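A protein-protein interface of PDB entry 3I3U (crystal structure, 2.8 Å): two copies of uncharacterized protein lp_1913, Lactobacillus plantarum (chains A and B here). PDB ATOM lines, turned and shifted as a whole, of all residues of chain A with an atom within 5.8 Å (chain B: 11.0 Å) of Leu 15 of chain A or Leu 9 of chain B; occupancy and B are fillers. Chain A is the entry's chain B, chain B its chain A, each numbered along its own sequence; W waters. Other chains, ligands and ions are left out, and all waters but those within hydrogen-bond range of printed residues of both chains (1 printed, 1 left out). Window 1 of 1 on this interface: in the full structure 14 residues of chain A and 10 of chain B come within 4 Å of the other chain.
Of the 15 printed residues of chain A, 9 touch a printed residue of chain B.
Printed residues of chain A that touch a printed residue of chain B: Thr 11, Tyr 12, Ser 14, Leu 15, Lys 87, Leu 90, Leu 91, Leu 94 and Tyr 101.
Hydrophobic or aromatic side chains of chain A within 4 Å of the printed part of chain B: Leu 15, Leu 90, Leu 91, Leu 94 and Tyr 101.
Printed residues of chain B that touch a printed residue of chain A: Lys 4, Lys 5, Ile 6, Leu 8, Leu 9, Thr 10, Tyr 12 and Leu 13.
Hydrophobic or aromatic side chains of chain B within 4 Å of the printed part of chain A: Ile 6, Leu 8, Leu 9, Tyr 12 and Leu 13.
Among the printed residues, 17 pairs touch across the chains.
Of chain B, only Lys 5 (3.6 Å), Leu 8 (3.8 Å) and Leu 9 (3.4 Å) come within 4 Å of Leu 15 of chain A.
Leu 9 of chain B touches just these residues of chain A: Leu 15, Lys 87, Leu 90 and Leu 94.
Of chain B, only Leu 8 (3.6 Å) comes within 4 Å of Tyr 12 of chain A.
Of chain B, only Lys 5 (3.2 Å) comes within 4 Å of Ser 14 of chain A.
Of chain B, only Leu 9 (3.6 Å), Tyr 12 (3.7 Å) and Leu 13 (3.9 Å) come within 4 Å of Lys 87 of chain A.
Printed residues of chain A within 4 Å of Ile 6 of chain B: Leu 91 and Leu 94.
Printed residues of chain B within 4 Å of Tyr 101 of chain A: Lys 5 (3.5 Å).
Of the printed residues of chain B, Leu 94 of chain A touches Lys 5 (3.7 Å), Ile 6 (3.5 Å) and Leu 9 (3.7 Å).
Glu 7 of chain B touches none of the printed residues of chain A.
The nearest residue of chain B that does not touch Leu 15 of chain A is Ile 6 of chain B (5.5 Å).
Among the printed residues, merely in contact across the chains: Thr 11 of chain A with Lys 4 of chain B, Thr 11 of chain A with Leu 8 of chain B, Tyr 12 of chain A with Leu 8 of chain B, Leu 15 of chain A with Lys 5 of chain B, Leu 15 of chain A with Leu 8 of chain B, Leu 15 of chain A with Leu 9 of chain B, Lys 87 of chain A with Leu 9 of chain B, Lys 87 of chain A with Tyr 12 of chain B, Lys 87 of chain A with Leu 13 of chain B, Leu 90 of chain A with Leu 9 of chain B, Leu 91 of chain A with Ile 6 of chain B, Leu 91 of chain A with Thr 10 of chain B, Leu 94 of chain A with Lys 5 of chain B, Leu 94 of chain A with Ile 6 of chain B, Leu 94 of chain A with Leu 9 of chain B and Tyr 101 of chain A with Lys 5 of chain B.
Water W1 lies within hydrogen-bond range of ND2 of Asn 2 of chain B and O of Leu 94 of chain A.
Positions printed for both chains: 10, 11, 12, 13, 14, 15 and 16.
The side-chain amino group (NZ) of Lys 5 of chain B sits at hydrogen-bond distance from the backbone carbonyl oxygen (O) of Ser 14 of chain A (3.2 Å).
The backbone carbonyl oxygen (O) of Ile 6 of chain B is in hydrogen-bond range of the side-chain hydroxyl (OG1) of Thr 10 of chain B, at 2.5 Å.
The side-chain hydroxyl (OH) of Tyr 12 of chain B is in hydrogen-bond range of the side-chain hydroxyl (OH) of Tyr 16 of chain B.
The backbone carbonyl oxygen (O) of Thr 10 of chain A is in hydrogen-bond range of the side-chain hydroxyl (OG) of Ser 14 of chain A, at 3.3 Å.
The side-chain hydroxyl (OG) of Ser 14 of chain A is in hydrogen-bond range of the backbone carbonyl oxygen (O) of Thr 11 of chain A (2.9 Å).
The side-chain hydroxyl of Tyr 16 of chain A sits at hydrogen-bond distance from the side-chain hydroxyl of Tyr 12 of chain A (3.1 Å).
The side-chain carboxylate of Glu 102 of chain A sits at hydrogen-bond distance from the backbone NH of Lys 87 of chain A, at 3.5 Å.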
ATOM      1  N   THR A  10     -16.202  -6.512  -1.464  1.00  0.00           N
ATOM      2  CA  THR A  10     -17.318  -7.222  -0.859  1.00  0.00           C
ATOM      3  C   THR A  10     -17.768  -6.529   0.426  1.00  0.00           C
ATOM      4  O   THR A  10     -18.955  -6.327   0.661  1.00  0.00           O
ATOM      5  CB  THR A  10     -16.936  -8.685  -0.523  1.00  0.00           C
ATOM      6  OG1 THR A  10     -16.678  -9.410  -1.725  1.00  0.00           O
ATOM      7  CG2 THR A  10     -18.048  -9.364   0.257  1.00  0.00           C
ATOM      8  N   THR A  11     -16.805  -6.173   1.269  1.00  0.00           N
ATOM      9  CA  THR A  11     -17.107  -5.512   2.526  1.00  0.00           C
ATOM     10  C   THR A  11     -17.500  -4.037   2.348  1.00  0.00           C
ATOM     11  O   THR A  11     -18.347  -3.507   3.081  1.00  0.00           O
ATOM     12  CB  THR A  11     -15.927  -5.652   3.466  1.00  0.00           C
ATOM     13  OG1 THR A  11     -15.785  -7.033   3.811  1.00  0.00           O
ATOM     14  CG2 THR A  11     -16.126  -4.816   4.730  1.00  0.00           C
ATOM     15  N   TYR A  12     -16.884  -3.373   1.372  1.00  0.00           N
ATOM     16  CA  TYR A  12     -17.229  -1.980   1.100  1.00  0.00           C
ATOM     17  C   TYR A  12     -18.691  -1.937   0.629  1.00  0.00           C
ATOM     18  O   TYR A  12     -19.477  -1.101   1.069  1.00  0.00           O
ATOM     19  CB  TYR A  12     -16.345  -1.402  -0.009  1.00  0.00           C
ATOM     20  CG  TYR A  12     -16.519   0.096  -0.187  1.00  0.00           C
ATOM     21  CD1 TYR A  12     -15.833   0.987   0.634  1.00  0.00           C
ATOM     22  CD2 TYR A  12     -17.406   0.619  -1.117  1.00  0.00           C
ATOM     23  CE1 TYR A  12     -16.025   2.345   0.542  1.00  0.00           C
ATOM     24  CE2 TYR A  12     -17.608   1.997  -1.215  1.00  0.00           C
ATOM     25  CZ  TYR A  12     -16.916   2.850  -0.373  1.00  0.00           C
ATOM     26  OH  TYR A  12     -17.124   4.213  -0.380  1.00  0.00           O
ATOM     27  N   LEU A  13     -19.038  -2.834  -0.280  1.00  0.00           N
ATOM     28  CA  LEU A  13     -20.415  -2.864  -0.805  1.00  0.00           C
ATOM     29  C   LEU A  13     -21.480  -3.297   0.206  1.00  0.00           C
ATOM     30  O   LEU A  13     -22.602  -2.795   0.168  1.00  0.00           O
ATOM     31  CB  LEU A  13     -20.488  -3.746  -2.060  1.00  0.00           C
ATOM     32  CG  LEU A  13     -19.657  -3.142  -3.189  1.00  0.00           C
ATOM     33  CD1 LEU A  13     -19.453  -4.174  -4.323  1.00  0.00           C
ATOM     34  CD2 LEU A  13     -20.331  -1.869  -3.689  1.00  0.00           C
ATOM     35  N   SER A  14     -21.136  -4.187   1.126  1.00  0.00           N
ATOM     36  CA  SER A  14     -22.119  -4.658   2.089  1.00  0.00           C
ATOM     37  C   SER A  14     -22.498  -3.576   3.060  1.00  0.00           C
ATOM     38  O   SER A  14     -23.321  -3.805   3.931  1.00  0.00           O
ATOM     39  CB  SER A  14     -21.570  -5.846   2.861  1.00  0.00           C
ATOM     40  OG  SER A  14     -20.386  -5.450   3.523  1.00  0.00           O
ATOM     41  N   LEU A  15     -21.883  -2.407   2.919  1.00  0.00           N
ATOM     42  CA  LEU A  15     -22.159  -1.265   3.785  1.00  0.00           C
ATOM     43  C   LEU A  15     -23.315  -0.469   3.216  1.00  0.00           C
ATOM     44  O   LEU A  15     -23.950   0.313   3.913  1.00  0.00           O
ATOM     45  CB  LEU A  15     -20.936  -0.352   3.884  1.00  0.00           C
ATOM     46  CG  LEU A  15     -19.667  -0.897   4.529  1.00  0.00           C
ATOM     47  CD1 LEU A  15     -18.516  -0.146   3.947  1.00  0.00           C
ATOM     48  CD2 LEU A  15     -19.693  -0.779   6.049  1.00  0.00           C
ATOM     49  N   TYR A  16     -23.595  -0.650   1.932  1.00  0.00           N
ATOM     50  CA  TYR A  16     -24.679   0.103   1.330  1.00  0.00           C
ATOM     51  C   TYR A  16     -25.950  -0.699   1.070  1.00  0.00           C
ATOM     52  O   TYR A  16     -25.929  -1.922   0.861  1.00  0.00           O
ATOM     53  CB  TYR A  16     -24.231   0.757   0.020  1.00  0.00           C
ATOM     54  CG  TYR A  16     -23.141   1.794   0.146  1.00  0.00           C
ATOM     55  CD1 TYR A  16     -21.800   1.417   0.152  1.00  0.00           C
ATOM     56  CD2 TYR A  16     -23.442   3.156   0.193  1.00  0.00           C
ATOM     57  CE1 TYR A  16     -20.790   2.363   0.188  1.00  0.00           C
ATOM     58  CE2 TYR A  16     -22.437   4.118   0.234  1.00  0.00           C
ATOM     59  CZ  TYR A  16     -21.113   3.710   0.227  1.00  0.00           C
ATOM     60  OH  TYR A  16     -20.097   4.639   0.239  1.00  0.00           O
ATOM     61  N   ILE A  17     -27.057   0.036   1.106  1.00  0.00           N
ATOM     62  CA  ILE A  17     -28.384  -0.491   0.856  1.00  0.00           C
ATOM     63  C   ILE A  17     -28.826   0.107  -0.480  1.00  0.00           C
ATOM     64  O   ILE A  17     -28.907   1.334  -0.651  1.00  0.00           O
ATOM     65  CB  ILE A  17     -29.380  -0.086   1.971  1.00  0.00           C
ATOM     66  CG1 ILE A  17     -30.799  -0.494   1.582  1.00  0.00           C
ATOM     67  CG2 ILE A  17     -29.331   1.408   2.203  1.00  0.00           C
ATOM     68  CD1 ILE A  17     -31.832  -0.132   2.618  1.00  0.00           C
ATOM     69  N   LYS A  87     -20.419   7.599   6.766  1.00  0.00           N
ATOM     70  CA  LYS A  87     -19.621   6.533   7.352  1.00  0.00           C
ATOM     71  C   LYS A  87     -19.561   6.607   8.862  1.00  0.00           C
ATOM     72  O   LYS A  87     -19.918   5.637   9.533  1.00  0.00           O
ATOM     73  CB  LYS A  87     -18.220   6.514   6.755  1.00  0.00           C
ATOM     74  CG  LYS A  87     -18.122   5.582   5.554  1.00  0.00           C
ATOM     75  CD  LYS A  87     -17.793   6.345   4.295  1.00  0.00           C
ATOM     76  CE  LYS A  87     -17.760   5.422   3.099  1.00  0.00           C
ATOM     77  NZ  LYS A  87     -16.678   4.404   3.261  1.00  0.00           N
ATOM     78  N   LEU A  90     -22.762   5.691  10.225  1.00  0.00           N
ATOM     79  CA  LEU A  90     -22.928   4.276   9.977  1.00  0.00           C
ATOM     80  C   LEU A  90     -22.134   3.488  11.006  1.00  0.00           C
ATOM     81  O   LEU A  90     -22.635   2.526  11.578  1.00  0.00           O
ATOM     82  CB  LEU A  90     -22.433   3.938   8.572  1.00  0.00           C
ATOM     83  CG  LEU A  90     -22.443   2.456   8.191  1.00  0.00           C
ATOM     84  CD1 LEU A  90     -23.874   1.908   8.227  1.00  0.00           C
ATOM     85  CD2 LEU A  90     -21.832   2.286   6.816  1.00  0.00           C
ATOM     86  N   LEU A  91     -20.885   3.903  11.237  1.00  0.00           N
ATOM     87  CA  LEU A  91     -20.022   3.238  12.214  1.00  0.00           C
ATOM     88  C   LEU A  91     -20.604   3.341  13.606  1.00  0.00           C
ATOM     89  O   LEU A  91     -20.459   2.424  14.406  1.00  0.00           O
ATOM     90  CB  LEU A  91     -18.615   3.840  12.213  1.00  0.00           C
ATOM     91  CG  LEU A  91     -17.650   3.441  13.350  1.00  0.00           C
ATOM     92  CD1 LEU A  91     -17.106   2.010  13.109  1.00  0.00           C
ATOM     93  CD2 LEU A  91     -16.477   4.430  13.413  1.00  0.00           C
ATOM     94  N   LEU A  94     -23.538   0.601  13.717  1.00  0.00           N
ATOM     95  CA  LEU A  94     -23.019  -0.765  13.677  1.00  0.00           C
ATOM     96  C   LEU A  94     -22.244  -1.120  14.951  1.00  0.00           C
ATOM     97  O   LEU A  94     -22.287  -2.261  15.402  1.00  0.00           O
ATOM     98  CB  LEU A  94     -22.127  -0.967  12.435  1.00  0.00           C
ATOM     99  CG  LEU A  94     -22.725  -0.751  11.027  1.00  0.00           C
ATOM    100  CD1 LEU A  94     -21.678  -1.017   9.932  1.00  0.00           C
ATOM    101  CD2 LEU A  94     -23.919  -1.673  10.835  1.00  0.00           C
ATOM    102  N   ALA A 100     -27.579  -1.387  10.265  1.00  0.00           N
ATOM    103  CA  ALA A 100     -27.681  -0.170   9.467  1.00  0.00           C
ATOM    104  C   ALA A 100     -26.929  -0.232   8.127  1.00  0.00           C
ATOM    105  O   ALA A 100     -26.025  -1.042   7.936  1.00  0.00           O
ATOM    106  CB  ALA A 100     -27.187   1.012  10.299  1.00  0.00           C
ATOM    107  N   TYR A 101     -27.315   0.625   7.192  1.00  0.00           N
ATOM    108  CA  TYR A 101     -26.676   0.663   5.888  1.00  0.00           C
ATOM    109  C   TYR A 101     -26.646   2.111   5.446  1.00  0.00           C
ATOM    110  O   TYR A 101     -27.333   2.949   6.018  1.00  0.00           O
ATOM    111  CB  TYR A 101     -27.477  -0.149   4.851  1.00  0.00           C
ATOM    112  CG  TYR A 101     -27.546  -1.639   5.107  1.00  0.00           C
ATOM    113  CD1 TYR A 101     -26.543  -2.500   4.652  1.00  0.00           C
ATOM    114  CD2 TYR A 101     -28.576  -2.176   5.877  1.00  0.00           C
ATOM    115  CE1 TYR A 101     -26.564  -3.860   4.972  1.00  0.00           C
ATOM    116  CE2 TYR A 101     -28.601  -3.528   6.204  1.00  0.00           C
ATOM    117  CZ  TYR A 101     -27.594  -4.363   5.753  1.00  0.00           C
ATOM    118  OH  TYR A 101     -27.602  -5.684   6.132  1.00  0.00           O
ATOM    119  N   GLU A 102     -25.842   2.414   4.435  1.00  0.00           N
ATOM    120  CA  GLU A 102     -25.795   3.761   3.904  1.00  0.00           C
ATOM    121  C   GLU A 102     -26.568   3.740   2.592  1.00  0.00           C
ATOM    122  O   GLU A 102     -26.475   2.776   1.819  1.00  0.00           O
ATOM    123  CB  GLU A 102     -24.357   4.200   3.655  1.00  0.00           C
ATOM    124  CG  GLU A 102     -24.241   5.610   3.107  1.00  0.00           C
ATOM    125  CD  GLU A 102     -22.822   6.134   3.170  1.00  0.00           C
ATOM    126  OE1 GLU A 102     -22.208   6.041   4.257  1.00  0.00           O
ATOM    127  OE2 GLU A 102     -22.318   6.638   2.141  1.00  0.00           O
ATOM    128  N   ASN B   2     -20.781  -7.942  11.887  1.00  0.00           N
ATOM    129  CA  ASN B   2     -20.382  -6.567  11.469  1.00  0.00           C
ATOM    130  C   ASN B   2     -18.916  -6.228  11.782  1.00  0.00           C
ATOM    131  O   ASN B   2     -18.486  -5.104  11.549  1.00  0.00           O
ATOM    132  CB  ASN B   2     -21.280  -5.515  12.142  1.00  0.00           C
ATOM    133  CG  ASN B   2     -22.759  -5.719  11.857  1.00  0.00           C
ATOM    134  OD1 ASN B   2     -23.160  -6.001  10.727  1.00  0.00           O
ATOM    135  ND2 ASN B   2     -23.583  -5.554  12.886  1.00  0.00           N
ATOM    136  N   ASP B   3     -18.147  -7.178  12.312  1.00  0.00           N
ATOM    137  CA  ASP B   3     -16.745  -6.899  12.635  1.00  0.00           C
ATOM    138  C   ASP B   3     -15.978  -6.432  11.401  1.00  0.00           C
ATOM    139  O   ASP B   3     -15.128  -5.543  11.484  1.00  0.00           O
ATOM    140  CB  ASP B   3     -16.067  -8.138  13.246  1.00  0.00           C
ATOM    141  CG  ASP B   3     -16.752  -8.612  14.527  1.00  0.00           C
ATOM    142  OD1 ASP B   3     -16.926  -7.791  15.462  1.00  0.00           O
ATOM    143  OD2 ASP B   3     -17.117  -9.809  14.598  1.00  0.00           O
ATOM    144  N   LYS B   4     -16.280  -7.022  10.244  1.00  0.00           N
ATOM    145  CA  LYS B   4     -15.619  -6.627   9.011  1.00  0.00           C
ATOM    146  C   LYS B   4     -16.000  -5.218   8.561  1.00  0.00           C
ATOM    147  O   LYS B   4     -15.150  -4.476   8.051  1.00  0.00           O
ATOM    148  CB  LYS B   4     -15.914  -7.633   7.908  1.00  0.00           C
ATOM    149  CG  LYS B   4     -15.096  -8.905   8.044  1.00  0.00           C
ATOM    150  CD  LYS B   4     -15.097  -9.676   6.744  1.00  0.00           C
ATOM    151  CE  LYS B   4     -14.084 -10.804   6.757  1.00  0.00           C
ATOM    152  NZ  LYS B   4     -12.703 -10.307   7.026  1.00  0.00           N
ATOM    153  N   LYS B   5     -17.261  -4.839   8.748  1.00  0.00           N
ATOM    154  CA  LYS B   5     -17.724  -3.503   8.369  1.00  0.00           C
ATOM    155  C   LYS B   5     -17.090  -2.464   9.287  1.00  0.00           C
ATOM    156  O   LYS B   5     -16.528  -1.466   8.834  1.00  0.00           O
ATOM    157  CB  LYS B   5     -19.241  -3.394   8.498  1.00  0.00           C
ATOM    158  CG  LYS B   5     -20.031  -4.292   7.588  1.00  0.00           C
ATOM    159  CD  LYS B   5     -21.512  -4.076   7.820  1.00  0.00           C
ATOM    160  CE  LYS B   5     -22.360  -5.019   6.991  1.00  0.00           C
ATOM    161  NZ  LYS B   5     -23.803  -4.597   6.984  1.00  0.00           N
ATOM    162  N   ILE B   6     -17.210  -2.698  10.589  1.00  0.00           N
ATOM    163  CA  ILE B   6     -16.654  -1.825  11.605  1.00  0.00           C
ATOM    164  C   ILE B   6     -15.142  -1.712  11.404  1.00  0.00           C
ATOM    165  O   ILE B   6     -14.566  -0.641  11.570  1.00  0.00           O
ATOM    166  CB  ILE B   6     -16.991  -2.374  13.002  1.00  0.00           C
ATOM    167  CG1 ILE B   6     -18.499  -2.278  13.224  1.00  0.00           C
ATOM    168  CG2 ILE B   6     -16.202  -1.635  14.078  1.00  0.00           C
ATOM    169  CD1 ILE B   6     -19.018  -3.091  14.397  1.00  0.00           C
ATOM    170  N   GLU B   7     -14.499  -2.813  11.014  1.00  0.00           N
ATOM    171  CA  GLU B   7     -13.059  -2.781  10.799  1.00  0.00           C
ATOM    172  C   GLU B   7     -12.703  -1.961   9.564  1.00  0.00           C
ATOM    173  O   GLU B   7     -11.685  -1.269   9.534  1.00  0.00           O
ATOM    174  CB  GLU B   7     -12.498  -4.196  10.682  1.00  0.00           C
ATOM    175  CG  GLU B   7     -10.983  -4.233  10.832  1.00  0.00           C
ATOM    176  CD  GLU B   7     -10.483  -3.230  11.884  1.00  0.00           C
ATOM    177  OE1 GLU B   7     -11.000  -3.245  13.028  1.00  0.00           O
ATOM    178  OE2 GLU B   7      -9.572  -2.423  11.562  1.00  0.00           O
ATOM    179  N   LEU B   8     -13.544  -2.017   8.532  1.00  0.00           N
ATOM    180  CA  LEU B   8     -13.277  -1.235   7.337  1.00  0.00           C
ATOM    181  C   LEU B   8     -13.623   0.250   7.553  1.00  0.00           C
ATOM    182  O   LEU B   8     -12.859   1.140   7.152  1.00  0.00           O
ATOM    183  CB  LEU B   8     -14.059  -1.798   6.166  1.00  0.00           C
ATOM    184  CG  LEU B   8     -14.103  -0.914   4.925  1.00  0.00           C
ATOM    185  CD1 LEU B   8     -12.706  -0.691   4.372  1.00  0.00           C
ATOM    186  CD2 LEU B   8     -15.026  -1.563   3.909  1.00  0.00           C
ATOM    187  N   LEU B   9     -14.746   0.529   8.208  1.00  0.00           N
ATOM    188  CA  LEU B   9     -15.148   1.912   8.446  1.00  0.00           C
ATOM    189  C   LEU B   9     -14.180   2.600   9.413  1.00  0.00           C
ATOM    190  O   LEU B   9     -13.833   3.774   9.245  1.00  0.00           O
ATOM    191  CB  LEU B   9     -16.577   1.951   8.997  1.00  0.00           C
ATOM    192  CG  LEU B   9     -17.638   1.364   8.065  1.00  0.00           C
ATOM    193  CD1 LEU B   9     -18.915   1.118   8.821  1.00  0.00           C
ATOM    194  CD2 LEU B   9     -17.884   2.305   6.906  1.00  0.00           C
ATOM    195  N   THR B  10     -13.731   1.856  10.413  1.00  0.00           N
ATOM    196  CA  THR B  10     -12.797   2.396  11.391  1.00  0.00           C
ATOM    197  C   THR B  10     -11.480   2.788  10.706  1.00  0.00           C
ATOM    198  O   THR B  10     -11.008   3.920  10.835  1.00  0.00           O
ATOM    199  CB  THR B  10     -12.539   1.360  12.503  1.00  0.00           C
ATOM    200  OG1 THR B  10     -13.778   1.082  13.174  1.00  0.00           O
ATOM    201  CG2 THR B  10     -11.505   1.861  13.495  1.00  0.00           C
ATOM    202  N   THR B  11     -10.893   1.862   9.949  1.00  0.00           N
ATOM    203  CA  THR B  11      -9.646   2.186   9.264  1.00  0.00           C
ATOM    204  C   THR B  11      -9.821   3.248   8.146  1.00  0.00           C
ATOM    205  O   THR B  11      -8.936   4.086   7.934  1.00  0.00           O
ATOM    206  CB  THR B  11      -9.006   0.927   8.682  1.00  0.00           C
ATOM    207  OG1 THR B  11      -8.647   0.058   9.758  1.00  0.00           O
ATOM    208  CG2 THR B  11      -7.763   1.283   7.860  1.00  0.00           C
ATOM    209  N   TYR B  12     -10.951   3.208   7.436  1.00  0.00           N
ATOM    210  CA  TYR B  12     -11.202   4.174   6.372  1.00  0.00           C
ATOM    211  C   TYR B  12     -11.227   5.592   6.951  1.00  0.00           C
ATOM    212  O   TYR B  12     -10.574   6.506   6.439  1.00  0.00           O
ATOM    213  CB  TYR B  12     -12.553   3.894   5.691  1.00  0.00           C
ATOM    214  CG  TYR B  12     -12.790   4.720   4.432  1.00  0.00           C
ATOM    215  CD1 TYR B  12     -12.260   4.318   3.207  1.00  0.00           C
ATOM    216  CD2 TYR B  12     -13.488   5.926   4.477  1.00  0.00           C
ATOM    217  CE1 TYR B  12     -12.404   5.092   2.077  1.00  0.00           C
ATOM    218  CE2 TYR B  12     -13.634   6.709   3.334  1.00  0.00           C
ATOM    219  CZ  TYR B  12     -13.080   6.284   2.141  1.00  0.00           C
ATOM    220  OH  TYR B  12     -13.159   7.057   1.009  1.00  0.00           O
ATOM    221  N   LEU B  13     -11.984   5.762   8.022  1.00  0.00           N
ATOM    222  CA  LEU B  13     -12.105   7.066   8.676  1.00  0.00           C
ATOM    223  C   LEU B  13     -10.835   7.529   9.380  1.00  0.00           C
ATOM    224  O   LEU B  13     -10.667   8.727   9.621  1.00  0.00           O
ATOM    225  CB  LEU B  13     -13.296   7.038   9.658  1.00  0.00           C
ATOM    226  CG  LEU B  13     -14.610   6.848   8.891  1.00  0.00           C
ATOM    227  CD1 LEU B  13     -15.753   6.386   9.813  1.00  0.00           C
ATOM    228  CD2 LEU B  13     -14.950   8.156   8.194  1.00  0.00           C
ATOM    229  N   SER B  14      -9.931   6.616   9.708  1.00  0.00           N
ATOM    230  CA  SER B  14      -8.716   7.035  10.404  1.00  0.00           C
ATOM    231  C   SER B  14      -7.819   7.767   9.427  1.00  0.00           C
ATOM    232  O   SER B  14      -6.826   8.363   9.808  1.00  0.00           O
ATOM    233  CB  SER B  14      -7.995   5.821  11.001  1.00  0.00           C
ATOM    234  OG  SER B  14      -7.389   5.040   9.990  1.00  0.00           O
ATOM    235  N   LEU B  15      -8.197   7.740   8.156  1.00  0.00           N
ATOM    236  CA  LEU B  15      -7.432   8.401   7.095  1.00  0.00           C
ATOM    237  C   LEU B  15      -7.752   9.877   6.967  1.00  0.00           C
ATOM    238  O   LEU B  15      -7.003  10.640   6.358  1.00  0.00           O
ATOM    239  CB  LEU B  15      -7.731   7.755   5.752  1.00  0.00           C
ATOM    240  CG  LEU B  15      -7.688   6.249   5.529  1.00  0.00           C
ATOM    241  CD1 LEU B  15      -8.291   6.018   4.165  1.00  0.00           C
ATOM    242  CD2 LEU B  15      -6.286   5.660   5.620  1.00  0.00           C
ATOM    243  N   TYR B  16      -8.882  10.300   7.513  1.00  0.00           N
ATOM    244  CA  TYR B  16      -9.232  11.697   7.375  1.00  0.00           C
ATOM    245  C   TYR B  16      -9.102  12.499   8.652  1.00  0.00           C
ATOM    246  O   TYR B  16      -9.105  11.963   9.763  1.00  0.00           O
ATOM    247  CB  TYR B  16     -10.652  11.844   6.827  1.00  0.00           C
ATOM    248  CG  TYR B  16     -10.897  11.225   5.472  1.00  0.00           C
ATOM    249  CD1 TYR B  16     -11.369   9.913   5.363  1.00  0.00           C
ATOM    250  CD2 TYR B  16     -10.743  11.968   4.294  1.00  0.00           C
ATOM    251  CE1 TYR B  16     -11.696   9.365   4.128  1.00  0.00           C
ATOM    252  CE2 TYR B  16     -11.064  11.426   3.046  1.00  0.00           C
ATOM    253  CZ  TYR B  16     -11.546  10.124   2.984  1.00  0.00           C
ATOM    254  OH  TYR B  16     -11.905   9.581   1.783  1.00  0.00           O
HETATM  255  O   HOH W   1     -24.249  -3.864  14.724  1.00  0.00           O
